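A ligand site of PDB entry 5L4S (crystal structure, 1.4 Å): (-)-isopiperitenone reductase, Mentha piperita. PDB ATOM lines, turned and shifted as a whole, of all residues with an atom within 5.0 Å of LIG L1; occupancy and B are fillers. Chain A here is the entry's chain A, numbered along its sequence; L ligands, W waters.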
ATOM      1  N   GLY A  14       3.437  -1.060  27.723  1.00  0.00           N
ATOM      2  CA  GLY A  14       3.923  -1.381  26.406  1.00  0.00           C
ATOM      3  C   GLY A  14       2.830  -1.356  25.370  1.00  0.00           C
ATOM      4  O   GLY A  14       2.640  -2.317  24.594  1.00  0.00           O
ATOM      5  N   ALA A  15       2.128  -0.221  25.292  1.00  0.00           N
ATOM      6  CA  ALA A  15       0.894  -0.115  24.538  1.00  0.00           C
ATOM      7  C   ALA A  15       0.992   0.741  23.288  1.00  0.00           C
ATOM      8  O   ALA A  15      -0.034   0.950  22.624  1.00  0.00           O
ATOM      9  CB  ALA A  15      -0.224   0.374  25.433  1.00  0.00           C
ATOM     10  N   ASN A  16       2.213   1.212  22.945  1.00  0.00           N
ATOM     11  CA  ASN A  16       2.339   2.007  21.724  1.00  0.00           C
ATOM     12  C   ASN A  16       2.303   1.170  20.466  1.00  0.00           C
ATOM     13  O   ASN A  16       2.109   1.727  19.400  1.00  0.00           O
ATOM     14  CB  ASN A  16       3.623   2.838  21.703  1.00  0.00           C
ATOM     15  CG  ASN A  16       4.861   2.024  21.936  1.00  0.00           C
ATOM     16  OD1 ASN A  16       5.097   1.521  23.041  1.00  0.00           O
ATOM     17  ND2 ASN A  16       5.672   1.876  20.875  1.00  0.00           N
ATOM     18  N   LYS A  17       2.460  -0.123  20.559  1.00  0.00           N
ATOM     19  CA  LYS A  17       2.467  -0.963  19.392  1.00  0.00           C
ATOM     20  C   LYS A  17       2.180  -2.388  19.818  1.00  0.00           C
ATOM     21  O   LYS A  17       2.045  -2.693  20.996  1.00  0.00           O
ATOM     22  CB  LYS A  17       3.785  -0.926  18.648  1.00  0.00           C
ATOM     23  CG  LYS A  17       5.008  -1.533  19.365  1.00  0.00           C
ATOM     24  CD  LYS A  17       6.285  -1.310  18.587  1.00  0.00           C
ATOM     25  CE  LYS A  17       7.470  -2.015  19.284  1.00  0.00           C
ATOM     26  NZ  LYS A  17       8.723  -1.865  18.491  1.00  0.00           N
ATOM     27  N   GLY A  18       2.105  -3.276  18.831  1.00  0.00           N
ATOM     28  CA  GLY A  18       1.985  -4.692  19.061  1.00  0.00           C
ATOM     29  C   GLY A  18       0.717  -5.052  19.791  1.00  0.00           C
ATOM     30  O   GLY A  18      -0.345  -4.421  19.641  1.00  0.00           O
ATOM     31  N   ILE A  19       0.800  -6.144  20.540  1.00  0.00           N
ATOM     32  CA  ILE A  19      -0.367  -6.663  21.245  1.00  0.00           C
ATOM     33  C   ILE A  19      -0.957  -5.632  22.173  1.00  0.00           C
ATOM     34  O   ILE A  19      -2.198  -5.532  22.298  1.00  0.00           O
ATOM     35  CB  ILE A  19       0.028  -7.942  21.998  1.00  0.00           C
ATOM     36  CG1 ILE A  19       0.496  -9.023  21.008  1.00  0.00           C
ATOM     37  CG2 ILE A  19      -1.182  -8.472  22.716  1.00  0.00           C
ATOM     38  CD1 ILE A  19       0.953 -10.292  21.654  1.00  0.00           C
ATOM     39  N   GLY A  20      -0.102  -4.867  22.872  1.00  0.00           N
ATOM     40  CA  GLY A  20      -0.586  -3.915  23.870  1.00  0.00           C
ATOM     41  C   GLY A  20      -1.492  -2.854  23.274  1.00  0.00           C
ATOM     42  O   GLY A  20      -2.495  -2.437  23.864  1.00  0.00           O
ATOM     43  N   SER A  38       3.444   4.028  27.592  1.00  0.00           N
ATOM     44  CA  SER A  38       4.609   3.642  26.807  1.00  0.00           C
ATOM     45  C   SER A  38       5.840   4.328  27.349  1.00  0.00           C
ATOM     46  O   SER A  38       5.751   5.365  27.993  1.00  0.00           O
ATOM     47  CB  SER A  38       4.433   3.938  25.342  1.00  0.00           C
ATOM     48  OG  SER A  38       4.466   5.268  25.116  1.00  0.00           O
ATOM     49  N   ARG A  39       6.980   3.706  27.134  1.00  0.00           N
ATOM     50  CA  ARG A  39       8.204   4.250  27.702  1.00  0.00           C
ATOM     51  C   ARG A  39       8.642   5.515  26.981  1.00  0.00           C
ATOM     52  O   ARG A  39       9.239   6.393  27.609  1.00  0.00           O
ATOM     53  CB  ARG A  39       9.314   3.213  27.734  1.00  0.00           C
ATOM     54  CG  ARG A  39       9.663   2.518  26.442  1.00  0.00           C
ATOM     55  CD  ARG A  39      10.927   1.687  26.623  1.00  0.00           C
ATOM     56  NE  ARG A  39      11.138   0.896  25.433  1.00  0.00           N
ATOM     57  CZ  ARG A  39      12.093  -0.005  25.283  1.00  0.00           C
ATOM     58  NH1 ARG A  39      12.998  -0.148  26.240  1.00  0.00           N
ATOM     59  NH2 ARG A  39      12.158  -0.714  24.154  1.00  0.00           N
ATOM     60  N   ASN A  40       8.433   5.579  25.653  1.00  0.00           N
ATOM     61  CA  ASN A  40       8.756   6.754  24.875  1.00  0.00           C
ATOM     62  C   ASN A  40       7.498   7.605  24.743  1.00  0.00           C
ATOM     63  O   ASN A  40       6.453   7.132  24.248  1.00  0.00           O
ATOM     64  CB  ASN A  40       9.306   6.343  23.498  1.00  0.00           C
ATOM     65  CG  ASN A  40       9.727   7.513  22.707  1.00  0.00           C
ATOM     66  OD1 ASN A  40       8.924   8.080  21.973  1.00  0.00           O
ATOM     67  ND2 ASN A  40      11.012   7.900  22.820  1.00  0.00           N
ATOM     68  N   ARG A  43       6.200   8.179  21.011  1.00  0.00           N
ATOM     69  CA  ARG A  43       5.525   6.990  20.469  1.00  0.00           C
ATOM     70  C   ARG A  43       4.161   6.786  21.105  1.00  0.00           C
ATOM     71  O   ARG A  43       3.211   6.388  20.435  1.00  0.00           O
ATOM     72  CB  ARG A  43       6.380   5.725  20.637  1.00  0.00           C
ATOM     73  CG  ARG A  43       7.567   5.739  19.708  1.00  0.00           C
ATOM     74  CD  ARG A  43       8.214   4.352  19.516  1.00  0.00           C
ATOM     75  NE  ARG A  43       8.956   3.841  20.663  1.00  0.00           N
ATOM     76  CZ  ARG A  43      10.214   4.164  20.955  1.00  0.00           C
ATOM     77  NH1 ARG A  43      10.883   5.066  20.199  1.00  0.00           N
ATOM     78  NH2 ARG A  43      10.814   3.614  22.019  1.00  0.00           N
ATOM     79  N   LEU A  67       5.304   5.512  30.802  1.00  0.00           N
ATOM     80  CA  LEU A  67       5.656   4.468  31.756  1.00  0.00           C
ATOM     81  C   LEU A  67       6.720   3.562  31.167  1.00  0.00           C
ATOM     82  O   LEU A  67       6.490   2.885  30.160  1.00  0.00           O
ATOM     83  CB  LEU A  67       4.446   3.655  32.134  1.00  0.00           C
ATOM     84  CG  LEU A  67       4.698   2.506  33.074  1.00  0.00           C
ATOM     85  CD1 LEU A  67       5.333   2.974  34.385  1.00  0.00           C
ATOM     86  CD2 LEU A  67       3.406   1.764  33.381  1.00  0.00           C
ATOM     87  N   ASP A  68       7.882   3.584  31.801  1.00  0.00           N
ATOM     88  CA  ASP A  68       8.955   2.634  31.539  1.00  0.00           C
ATOM     89  C   ASP A  68       9.002   1.748  32.776  1.00  0.00           C
ATOM     90  O   ASP A  68       9.285   2.212  33.885  1.00  0.00           O
ATOM     91  CB  ASP A  68      10.273   3.355  31.280  1.00  0.00           C
ATOM     92  CG  ASP A  68      11.428   2.423  31.013  1.00  0.00           C
ATOM     93  OD1 ASP A  68      11.419   1.275  31.479  1.00  0.00           O
ATOM     94  OD2 ASP A  68      12.390   2.878  30.346  1.00  0.00           O
ATOM     95  N   VAL A  69       8.686   0.477  32.578  1.00  0.00           N
ATOM     96  CA  VAL A  69       8.528  -0.450  33.692  1.00  0.00           C
ATOM     97  C   VAL A  69       9.842  -0.823  34.344  1.00  0.00           C
ATOM     98  O   VAL A  69       9.831  -1.515  35.376  1.00  0.00           O
ATOM     99  CB  VAL A  69       7.770  -1.714  33.262  1.00  0.00           C
ATOM    100  CG1 VAL A  69       6.447  -1.362  32.670  1.00  0.00           C
ATOM    101  CG2 VAL A  69       8.548  -2.582  32.278  1.00  0.00           C
ATOM    102  N   THR A  70      10.972  -0.375  33.773  1.00  0.00           N
ATOM    103  CA  THR A  70      12.287  -0.595  34.372  1.00  0.00           C
ATOM    104  C   THR A  70      12.804   0.617  35.134  1.00  0.00           C
ATOM    105  O   THR A  70      13.915   0.560  35.692  1.00  0.00           O
ATOM    106  CB  THR A  70      13.345  -0.973  33.310  1.00  0.00           C
ATOM    107  OG1 THR A  70      13.678   0.183  32.508  1.00  0.00           O
ATOM    108  CG2 THR A  70      12.902  -2.091  32.405  1.00  0.00           C
ATOM    109  N   ASN A  95       1.948  -6.008  29.919  1.00  0.00           N
ATOM    110  CA  ASN A  95       2.177  -6.452  28.559  1.00  0.00           C
ATOM    111  C   ASN A  95       3.587  -6.168  28.062  1.00  0.00           C
ATOM    112  O   ASN A  95       4.133  -6.935  27.272  1.00  0.00           O
ATOM    113  CB  ASN A  95       1.141  -5.816  27.633  1.00  0.00           C
ATOM    114  CG  ASN A  95       1.494  -6.003  26.175  1.00  0.00           C
ATOM    115  OD1 ASN A  95       1.222  -7.058  25.573  1.00  0.00           O
ATOM    116  ND2 ASN A  95       2.080  -4.982  25.583  1.00  0.00           N
ATOM    117  N   ALA A  96       4.204  -5.073  28.488  1.00  0.00           N
ATOM    118  CA  ALA A  96       5.536  -4.745  28.019  1.00  0.00           C
ATOM    119  C   ALA A  96       6.481  -5.948  28.149  1.00  0.00           C
ATOM    120  O   ALA A  96       6.506  -6.635  29.156  1.00  0.00           O
ATOM    121  CB  ALA A  96       6.102  -3.572  28.832  1.00  0.00           C
ATOM    122  N   GLY A  97       7.336  -6.130  27.156  1.00  0.00           N
ATOM    123  CA  GLY A  97       8.321  -7.179  27.199  1.00  0.00           C
ATOM    124  C   GLY A  97       9.323  -7.034  26.081  1.00  0.00           C
ATOM    125  O   GLY A  97       9.031  -6.398  25.056  1.00  0.00           O
ATOM    126  N   VAL A  98      10.514  -7.573  26.314  1.00  0.00           N
ATOM    127  CA  VAL A  98      11.573  -7.640  25.331  1.00  0.00           C
ATOM    128  C   VAL A  98      12.150  -9.051  25.292  1.00  0.00           C
ATOM    129  O   VAL A  98      11.988  -9.820  26.229  1.00  0.00           O
ATOM    130  CB  VAL A  98      12.672  -6.612  25.626  1.00  0.00           C
ATOM    131  CG1 VAL A  98      12.140  -5.259  25.610  1.00  0.00           C
ATOM    132  CG2 VAL A  98      13.367  -6.881  26.938  1.00  0.00           C
ATOM    133  N   THR A 155      12.769  -6.065  32.526  1.00  0.00           N
ATOM    134  CA  THR A 155      11.514  -5.653  31.901  1.00  0.00           C
ATOM    135  C   THR A 155      10.409  -6.669  32.139  1.00  0.00           C
ATOM    136  O   THR A 155       9.276  -6.301  32.422  1.00  0.00           O
ATOM    137  CB  THR A 155      11.707  -5.522  30.393  1.00  0.00           C
ATOM    138  OG1 THR A 155      12.785  -4.633  30.115  1.00  0.00           O
ATOM    139  CG2 THR A 155      10.446  -4.994  29.736  1.00  0.00           C
ATOM    140  N   ASN A 156      10.707  -7.944  31.958  1.00  0.00           N
ATOM    141  CA  ASN A 156       9.675  -8.981  31.841  1.00  0.00           C
ATOM    142  C   ASN A 156       9.258  -9.553  33.172  1.00  0.00           C
ATOM    143  O   ASN A 156       8.151 -10.070  33.279  1.00  0.00           O
ATOM    144  CB  ASN A 156      10.166 -10.120  30.944  1.00  0.00           C
ATOM    145  CG  ASN A 156      10.327  -9.738  29.482  1.00  0.00           C
ATOM    146  OD1 ASN A 156      10.331  -8.602  29.096  1.00  0.00           O
ATOM    147  ND2 ASN A 156      10.477 -10.773  28.657  1.00  0.00           N
ATOM    148  N   VAL A 182       1.063 -10.779  30.648  1.00  0.00           N
ATOM    149  CA  VAL A 182       1.246 -11.353  29.330  1.00  0.00           C
ATOM    150  C   VAL A 182       2.547 -12.144  29.354  1.00  0.00           C
ATOM    151  O   VAL A 182       3.651 -11.582  29.363  1.00  0.00           O
ATOM    152  CB  VAL A 182       1.242 -10.313  28.227  1.00  0.00           C
ATOM    153  CG1 VAL A 182       1.403 -10.975  26.857  1.00  0.00           C
ATOM    154  CG2 VAL A 182       0.023  -9.456  28.292  1.00  0.00           C
ATOM    155  N   SER A 183       2.407 -13.454  29.387  1.00  0.00           N
ATOM    156  CA  SER A 183       3.534 -14.350  29.584  1.00  0.00           C
ATOM    157  C   SER A 183       3.726 -15.171  28.322  1.00  0.00           C
ATOM    158  O   SER A 183       3.392 -14.709  27.225  1.00  0.00           O
ATOM    159  CB  SER A 183       3.304 -15.156  30.866  1.00  0.00           C
ATOM    160  OG  SER A 183       4.485 -15.926  31.122  1.00  0.00           O
ATOM    161  N   SER A 184       4.238 -16.385  28.481  1.00  0.00           N
ATOM    162  CA  SER A 184       4.497 -17.242  27.329  1.00  0.00           C
ATOM    163  C   SER A 184       4.474 -18.665  27.788  1.00  0.00           C
ATOM    164  O   SER A 184       4.936 -18.976  28.870  1.00  0.00           O
ATOM    165  CB  SER A 184       5.860 -16.968  26.679  1.00  0.00           C
ATOM    166  OG  SER A 184       6.088 -17.967  25.700  1.00  0.00           O
ATOM    167  N   GLU A 240      14.570 -15.044  28.110  1.00  0.00           N
ATOM    168  CA  GLU A 240      13.131 -15.028  27.887  1.00  0.00           C
ATOM    169  C   GLU A 240      12.454 -16.118  28.718  1.00  0.00           C
ATOM    170  O   GLU A 240      11.439 -15.885  29.392  1.00  0.00           O
ATOM    171  CB  GLU A 240      12.814 -15.232  26.402  1.00  0.00           C
ATOM    172  CG  GLU A 240      12.715 -13.959  25.596  1.00  0.00           C
ATOM    173  CD  GLU A 240      11.342 -13.236  25.728  1.00  0.00           C
ATOM    174  OE1 GLU A 240      10.711 -13.284  26.779  1.00  0.00           O
ATOM    175  OE2 GLU A 240      10.831 -12.675  24.720  1.00  0.00           O
ATOM    176  N   LYS A 244       9.895 -15.359  31.886  1.00  0.00           N
ATOM    177  CA  LYS A 244       8.488 -15.709  31.823  1.00  0.00           C
ATOM    178  C   LYS A 244       8.152 -16.767  32.876  1.00  0.00           C
ATOM    179  O   LYS A 244       7.058 -16.746  33.447  1.00  0.00           O
ATOM    180  CB  LYS A 244       8.085 -16.148  30.428  1.00  0.00           C
ATOM    181  CG  LYS A 244       8.228 -15.054  29.361  1.00  0.00           C
ATOM    182  CD  LYS A 244       7.368 -13.803  29.603  1.00  0.00           C
ATOM    183  CE  LYS A 244       7.244 -13.036  28.307  1.00  0.00           C
ATOM    184  NZ  LYS A 244       6.447 -11.765  28.527  1.00  0.00           N
ATOM    185  N   CYS A 267      -0.744 -16.819  27.643  1.00  0.00           N
ATOM    186  CA  CYS A 267      -0.010 -16.839  26.382  1.00  0.00           C
ATOM    187  C   CYS A 267      -0.991 -16.377  25.324  1.00  0.00           C
ATOM    188  O   CYS A 267      -2.067 -17.000  25.202  1.00  0.00           O
ATOM    189  CB  CYS A 267       0.569 -18.207  26.010  1.00  0.00           C
ATOM    190  SG  CYS A 267       1.652 -18.078  24.546  1.00  0.00           S
ATOM    191  N   PRO A 268      -0.681 -15.304  24.567  1.00  0.00           N
ATOM    192  CA  PRO A 268      -1.641 -14.785  23.594  1.00  0.00           C
ATOM    193  C   PRO A 268      -1.672 -15.567  22.308  1.00  0.00           C
ATOM    194  O   PRO A 268      -2.577 -15.326  21.494  1.00  0.00           O
ATOM    195  CB  PRO A 268      -1.129 -13.343  23.362  1.00  0.00           C
ATOM    196  CG  PRO A 268       0.390 -13.479  23.529  1.00  0.00           C
ATOM    197  CD  PRO A 268       0.512 -14.432  24.680  1.00  0.00           C
ATOM    198  N   GLY A 269      -0.684 -16.449  22.085  1.00  0.00           N
ATOM    199  CA  GLY A 269      -0.455 -17.111  20.833  1.00  0.00           C
ATOM    200  C   GLY A 269       0.697 -16.450  20.107  1.00  0.00           C
ATOM    201  O   GLY A 269       1.152 -15.375  20.480  1.00  0.00           O
ATOM    202  N   TYR A 270       1.121 -17.068  19.018  1.00  0.00           N
ATOM    203  CA  TYR A 270       2.262 -16.600  18.245  1.00  0.00           C
ATOM    204  C   TYR A 270       1.755 -15.620  17.202  1.00  0.00           C
ATOM    205  O   TYR A 270       1.009 -15.988  16.296  1.00  0.00           O
ATOM    206  CB  TYR A 270       2.917 -17.833  17.639  1.00  0.00           C
ATOM    207  CG  TYR A 270       4.166 -17.615  16.799  1.00  0.00           C
ATOM    208  CD1 TYR A 270       4.948 -16.488  16.922  1.00  0.00           C
ATOM    209  CD2 TYR A 270       4.572 -18.593  15.898  1.00  0.00           C
ATOM    210  CE1 TYR A 270       6.097 -16.318  16.157  1.00  0.00           C
ATOM    211  CE2 TYR A 270       5.724 -18.451  15.144  1.00  0.00           C
ATOM    212  CZ  TYR A 270       6.463 -17.311  15.260  1.00  0.00           C
ATOM    213  OH  TYR A 270       7.603 -17.167  14.513  1.00  0.00           O
ATOM    214  N   ALA A 271       2.120 -14.369  17.388  1.00  0.00           N
ATOM    215  CA  ALA A 271       1.478 -13.262  16.689  1.00  0.00           C
ATOM    216  C   ALA A 271       2.501 -12.367  15.996  1.00  0.00           C
ATOM    217  O   ALA A 271       3.613 -12.180  16.458  1.00  0.00           O
ATOM    218  CB  ALA A 271       0.690 -12.432  17.662  1.00  0.00           C
ATOM    219  N   THR A 273       4.323  -9.374  15.365  1.00  0.00           N
ATOM    220  CA  THR A 273       4.674  -8.094  15.966  1.00  0.00           C
ATOM    221  C   THR A 273       6.162  -7.840  15.757  1.00  0.00           C
ATOM    222  O   THR A 273       6.900  -8.707  15.234  1.00  0.00           O
ATOM    223  CB  THR A 273       4.401  -8.086  17.467  1.00  0.00           C
ATOM    224  OG1 THR A 273       5.329  -9.003  18.063  1.00  0.00           O
ATOM    225  CG2 THR A 273       2.964  -8.469  17.803  1.00  0.00           C
ATOM    226  N   ASP A 274       6.647  -6.665  16.182  1.00  0.00           N
ATOM    227  CA  ASP A 274       8.070  -6.408  16.028  1.00  0.00           C
ATOM    228  C   ASP A 274       8.916  -7.461  16.747  1.00  0.00           C
ATOM    229  O   ASP A 274      10.005  -7.804  16.265  1.00  0.00           O
ATOM    230  CB  ASP A 274       8.416  -5.011  16.543  1.00  0.00           C
ATOM    231  CG  ASP A 274       8.051  -3.941  15.576  1.00  0.00           C
ATOM    232  OD1 ASP A 274       7.979  -4.205  14.360  1.00  0.00           O
ATOM    233  OD2 ASP A 274       7.924  -2.781  15.990  1.00  0.00           O
ATOM    234  N   ILE A 275       8.433  -7.993  17.869  1.00  0.00           N
ATOM    235  CA  ILE A 275       9.276  -8.894  18.644  1.00  0.00           C
ATOM    236  C   ILE A 275       9.490 -10.191  17.874  1.00  0.00           C
ATOM    237  O   ILE A 275      10.489 -10.892  18.086  1.00  0.00           O
ATOM    238  CB  ILE A 275       8.713  -9.122  20.075  1.00  0.00           C
ATOM    239  CG1 ILE A 275       9.860  -9.488  21.049  1.00  0.00           C
ATOM    240  CG2 ILE A 275       7.623 -10.206  20.077  1.00  0.00           C
ATOM    241  CD1 ILE A 275       9.389  -9.520  22.538  1.00  0.00           C
ATOM    242  N   THR A 276       8.572 -10.554  16.981  1.00  0.00           N
ATOM    243  CA  THR A 276       8.690 -11.789  16.206  1.00  0.00           C
ATOM    244  C   THR A 276       9.077 -11.494  14.754  1.00  0.00           C
ATOM    245  O   THR A 276       8.982 -12.385  13.905  1.00  0.00           O
ATOM    246  CB  THR A 276       7.381 -12.568  16.202  1.00  0.00           C
ATOM    247  OG1 THR A 276       6.358 -11.813  15.524  1.00  0.00           O
ATOM    248  CG2 THR A 276       6.968 -12.960  17.581  1.00  0.00           C
HETATM  249  P1  LIG L   1       6.332  -5.654  20.454  1.00  0.00           P
HETATM  250  O1  LIG L   1       7.739  -5.655  20.475  1.00  0.00           O
HETATM  251  O2  LIG L   1       5.529  -5.306  19.269  1.00  0.00           O
HETATM  252  O3  LIG L   1       5.764  -4.736  21.669  1.00  0.00           O
HETATM  253  C1  LIG L   1       6.475  -4.650  22.862  1.00  0.00           C
HETATM  254  C2  LIG L   1       5.913  -3.407  23.602  1.00  0.00           C
HETATM  255  O4  LIG L   1       6.671  -3.499  24.936  1.00  0.00           O
HETATM  256  C3  LIG L   1       6.312  -2.231  23.000  1.00  0.00           C
HETATM  257  O5  LIG L   1       5.288  -1.224  23.224  1.00  0.00           O
HETATM  258  C4  LIG L   1       7.612  -1.831  23.783  1.00  0.00           C
HETATM  259  O6  LIG L   1       7.858  -0.373  23.653  1.00  0.00           O
HETATM  260  C5  LIG L   1       7.246  -2.108  25.081  1.00  0.00           C
HETATM  261  N1  LIG L   1       8.383  -2.157  25.985  1.00  0.00           N
HETATM  262  C6  LIG L   1       9.583  -2.763  25.959  1.00  0.00           C
HETATM  263  N2  LIG L   1      10.320  -2.442  26.999  1.00  0.00           N
HETATM  264  C7  LIG L   1       9.476  -1.606  27.700  1.00  0.00           C
HETATM  265  C8  LIG L   1       9.778  -0.959  28.883  1.00  0.00           C
HETATM  266  N3  LIG L   1      10.911  -0.967  29.672  1.00  0.00           N
HETATM  267  N4  LIG L   1       8.837  -0.160  29.490  1.00  0.00           N
HETATM  268  C9  LIG L   1       7.695  -0.042  28.825  1.00  0.00           C
HETATM  269  N5  LIG L   1       7.344  -0.623  27.659  1.00  0.00           N
HETATM  270  C10 LIG L   1       8.313  -1.425  27.116  1.00  0.00           C
HETATM  271  O7  LIG L   1       5.927  -7.171  20.932  1.00  0.00           O
HETATM  272  P2  LIG L   1       4.587  -7.841  21.386  1.00  0.00           P
HETATM  273  O8  LIG L   1       4.535  -9.160  20.700  1.00  0.00           O
HETATM  274  O9  LIG L   1       3.408  -6.998  21.237  1.00  0.00           O
HETATM  275  O10 LIG L   1       4.970  -8.003  22.965  1.00  0.00           O
HETATM  276  C11 LIG L   1       3.915  -7.827  23.922  1.00  0.00           C
HETATM  277  C12 LIG L   1       4.099  -8.944  24.995  1.00  0.00           C
HETATM  278  O11 LIG L   1       3.550 -10.199  24.326  1.00  0.00           O
HETATM  279  C13 LIG L   1       5.386  -9.202  25.422  1.00  0.00           C
HETATM  280  O12 LIG L   1       5.429  -9.342  26.915  1.00  0.00           O
HETATM  281  C14 LIG L   1       5.796 -10.585  24.841  1.00  0.00           C
HETATM  282  O13 LIG L   1       6.694 -11.269  25.632  1.00  0.00           O
HETATM  283  C15 LIG L   1       4.436 -11.158  24.771  1.00  0.00           C
HETATM  284  N6  LIG L   1       4.255 -12.297  23.840  1.00  0.00           N
HETATM  285  C16 LIG L   1       4.303 -12.098  22.498  1.00  0.00           C
HETATM  286  C17 LIG L   1       4.124 -13.148  21.657  1.00  0.00           C
HETATM  287  C18 LIG L   1       4.109 -13.058  20.136  1.00  0.00           C
HETATM  288  O14 LIG L   1       4.096 -13.984  19.423  1.00  0.00           O
HETATM  289  N7  LIG L   1       4.089 -11.760  19.565  1.00  0.00           N
HETATM  290  C19 LIG L   1       3.857 -14.406  22.118  1.00  0.00           C
HETATM  291  C20 LIG L   1       3.838 -14.598  23.467  1.00  0.00           C
HETATM  292  C21 LIG L   1       4.007 -13.566  24.322  1.00  0.00           C
HETATM  293  P3  LIG L   1       8.906   0.298  22.540  1.00  0.00           P
HETATM  294  O15 LIG L   1       9.426   1.461  23.287  1.00  0.00           O
HETATM  295  O16 LIG L   1       8.110   0.591  21.376  1.00  0.00           O
HETATM  296  O17 LIG L   1       9.999  -0.734  22.312  1.00  0.00           O
HETATM  297  C1  LG2 L   2       8.069 -13.589  24.135  1.00  0.00           C
HETATM  298  C2  LG2 L   2       9.092 -15.967  25.777  1.00  0.00           C
HETATM  299  C3  LG2 L   2       9.537 -15.887  24.308  1.00  0.00           C
HETATM  300  C4  LG2 L   2       9.064 -14.627  23.506  1.00  0.00           C
HETATM  301  C5  LG2 L   2       9.336 -14.599  22.069  1.00  0.00           C
HETATM  302  C6  LG2 L   2      10.596 -15.591  21.668  1.00  0.00           C
HETATM  303  C7  LG2 L   2      10.492 -16.885  22.179  1.00  0.00           C
HETATM  304  C8  LG2 L   2      10.518 -16.843  23.811  1.00  0.00           C
HETATM  305  C9  LG2 L   2       8.103 -14.940  21.164  1.00  0.00           C
HETATM  306  C10 LG2 L   2       9.743 -13.166  21.709  1.00  0.00           C
HETATM  307  O1  LG2 L   2       6.930 -14.159  24.196  1.00  0.00           O
HETATM  308  O   HOH W   1       9.884  -5.954  22.446  1.00  0.00           O
HETATM  309  O   HOH W   2       6.358   1.243  25.767  1.00  0.00           O
HETATM  310  O   HOH W   3       2.756  -4.844  22.742  1.00  0.00           O
HETATM  311  O   HOH W   4      12.910  -2.724  28.173  1.00  0.00           O
HETATM  312  O   HOH W   5       9.109   0.906  18.888  1.00  0.00           O
HETATM  313  O   HOH W   6       9.879  -4.144  19.819  1.00  0.00           O
HETATM  314  O   HOH W   7       4.930  -4.510  16.887  1.00  0.00           O
HETATM  315  O   HOH W   8      11.969  -0.146  20.609  1.00  0.00           O
HETATM  316  O   HOH W   9      10.750  -3.314  22.547  1.00  0.00           O
HETATM  317  O   HOH W  10       7.543   3.430  23.734  1.00  0.00           O
HETATM  318  O   HOH W  11       6.167 -16.716  23.414  1.00  0.00           O
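N of Gly 20 lies close to ND2 of Asn 95, 3.5 Å away.
OG1 of Thr 273 sits close to N of Ile 275, at 3.3 Å.
The backbone NH (N) of Arg 43 sits at hydrogen-bond distance from the side-chain amide oxygen (OD1) of Asn 40, 2.9 Å away.
The side-chain hydroxyl of Thr 276 lies within hydrogen-bond range of the backbone carbonyl oxygen of Ala 271 (2.9 Å).
OD1 of Asp 68 is in hydrogen-bond range of OG1 of Thr 70, 2.7 Å away.
NZ of Lys 17 lies within salt-bridge range of OD2 of Asp 274, at 2.8 Å.
The backbone carbonyl oxygen of Ser 38 is in hydrogen-bond range of the backbone NH of Leu 67, at 2.8 Å.
The side-chain amide oxygen (OD1) of Asn 156 sits at hydrogen-bond distance from the backbone NH (N) of Val 98, at 3.0 Å.
The backbone carbonyl oxygen (O) of Asn 95 is in hydrogen-bond range of an oxygen (O12) of LIG L1 (2.8 Å).
The side-chain amide oxygen of Asn 16 sits at hydrogen-bond distance from an oxygen (O5) of LIG L1 (2.8 Å).
The side-chain hydroxyl (OG1) of Thr 273 lies within hydrogen-bond range of an oxygen (O8) of LIG L1, at 2.8 Å.
O15 of LIG L1 lies within salt-bridge range of NE of Arg 39.
The backbone NH (N) of Ile 19 sits at hydrogen-bond distance from an oxygen (O9) of LIG L1, 2.8 Å away.
The guanidinium group (NH2) of Arg 43 is in salt-bridge range of an oxygen (O15) of LIG L1, at 2.9 Å.
The backbone NH (N) of Ala 271 sits at hydrogen-bond distance from an oxygen (O14) of LIG L1, 2.9 Å away.
The backbone carbonyl oxygen (O) of Ala 271 lies within hydrogen-bond range of a nitrogen (N7) of LIG L1, 3.2 Å away.
N3 of LIG L1 is in hydrogen-bond range of OD1 of Asp 68 (2.9 Å).
NZ of Lys 244 lies within hydrogen-bond range of O13 of LIG L1 (2.9 Å).
N of Val 69 is in hydrogen-bond range of N4 of LIG L1 (3.2 Å).
O of Gly 14 is in hydrogen-bond range of O5 of LIG L1 (3.2 Å).
O16 of LIG L1 lies within salt-bridge range of NZ of Lys 17 (3.8 Å).
The backbone carbonyl oxygen of Gly 269 lies close to an oxygen (O14) of LIG L1 (3.4 Å).
Merely in contact with LIG L1: Ser 183 (3.2 Å), Ile 275 (3.3 Å), Tyr 270 (3.4 Å), Ala 96 (3.4 Å), Val 182 (3.4 Å), Leu 67 (3.4 Å), Gly 18 (3.5 Å), Gly 97 (3.5 Å), Pro 268 (3.5 Å), Asp 274 (3.6 Å), Thr 276 (3.6 Å), Thr 70 (3.6 Å), Val 98 (3.6 Å), Thr 155 (3.7 Å) and Ala 15 (3.9 Å).
Hydrophobic or aromatic side chains that line LIG L1: Ile 19, Val 69, Ala 96, Val 98, Val 182, Pro 268, Tyr 270, Ala 271 and Ile 275.
Of the 35 residues printed, 28 come within 4 Å of LIG L1.
The nearest printed residue that does not touch LIG L1 is Cys 267 (4.2 Å).
An oxygen (O1) of LG2 L2 sits close to an oxygen (O13) of LIG L1 (3.2 Å).
Water W7 bridges O2 of LIG L1 (2.6 Å) and N of Asp 274 (2.8 Å).
Water W9 bridges an oxygen (O17) of LIG L1 (2.7 Å) and the guanidinium group (NH2) of Arg 39 (3.4 Å).
Water W6 bridges an oxygen (O1) of LIG L1 and the side-chain amino group (NZ) of Lys 17.
Water W4 lies within hydrogen-bond range of the side-chain hydroxyl of Thr 155, a nitrogen (N2) of LIG L1 and the guanidinium group of Arg 39.
Water W1 lies within hydrogen-bond range of O of Gly 97 (2.8 Å) and O1 of LIG L1 (2.9 Å).
Water W11 bridges the side-chain hydroxyl of Ser 184 (2.6 Å) and an oxygen (O1) of LG2 L2 (2.8 Å).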
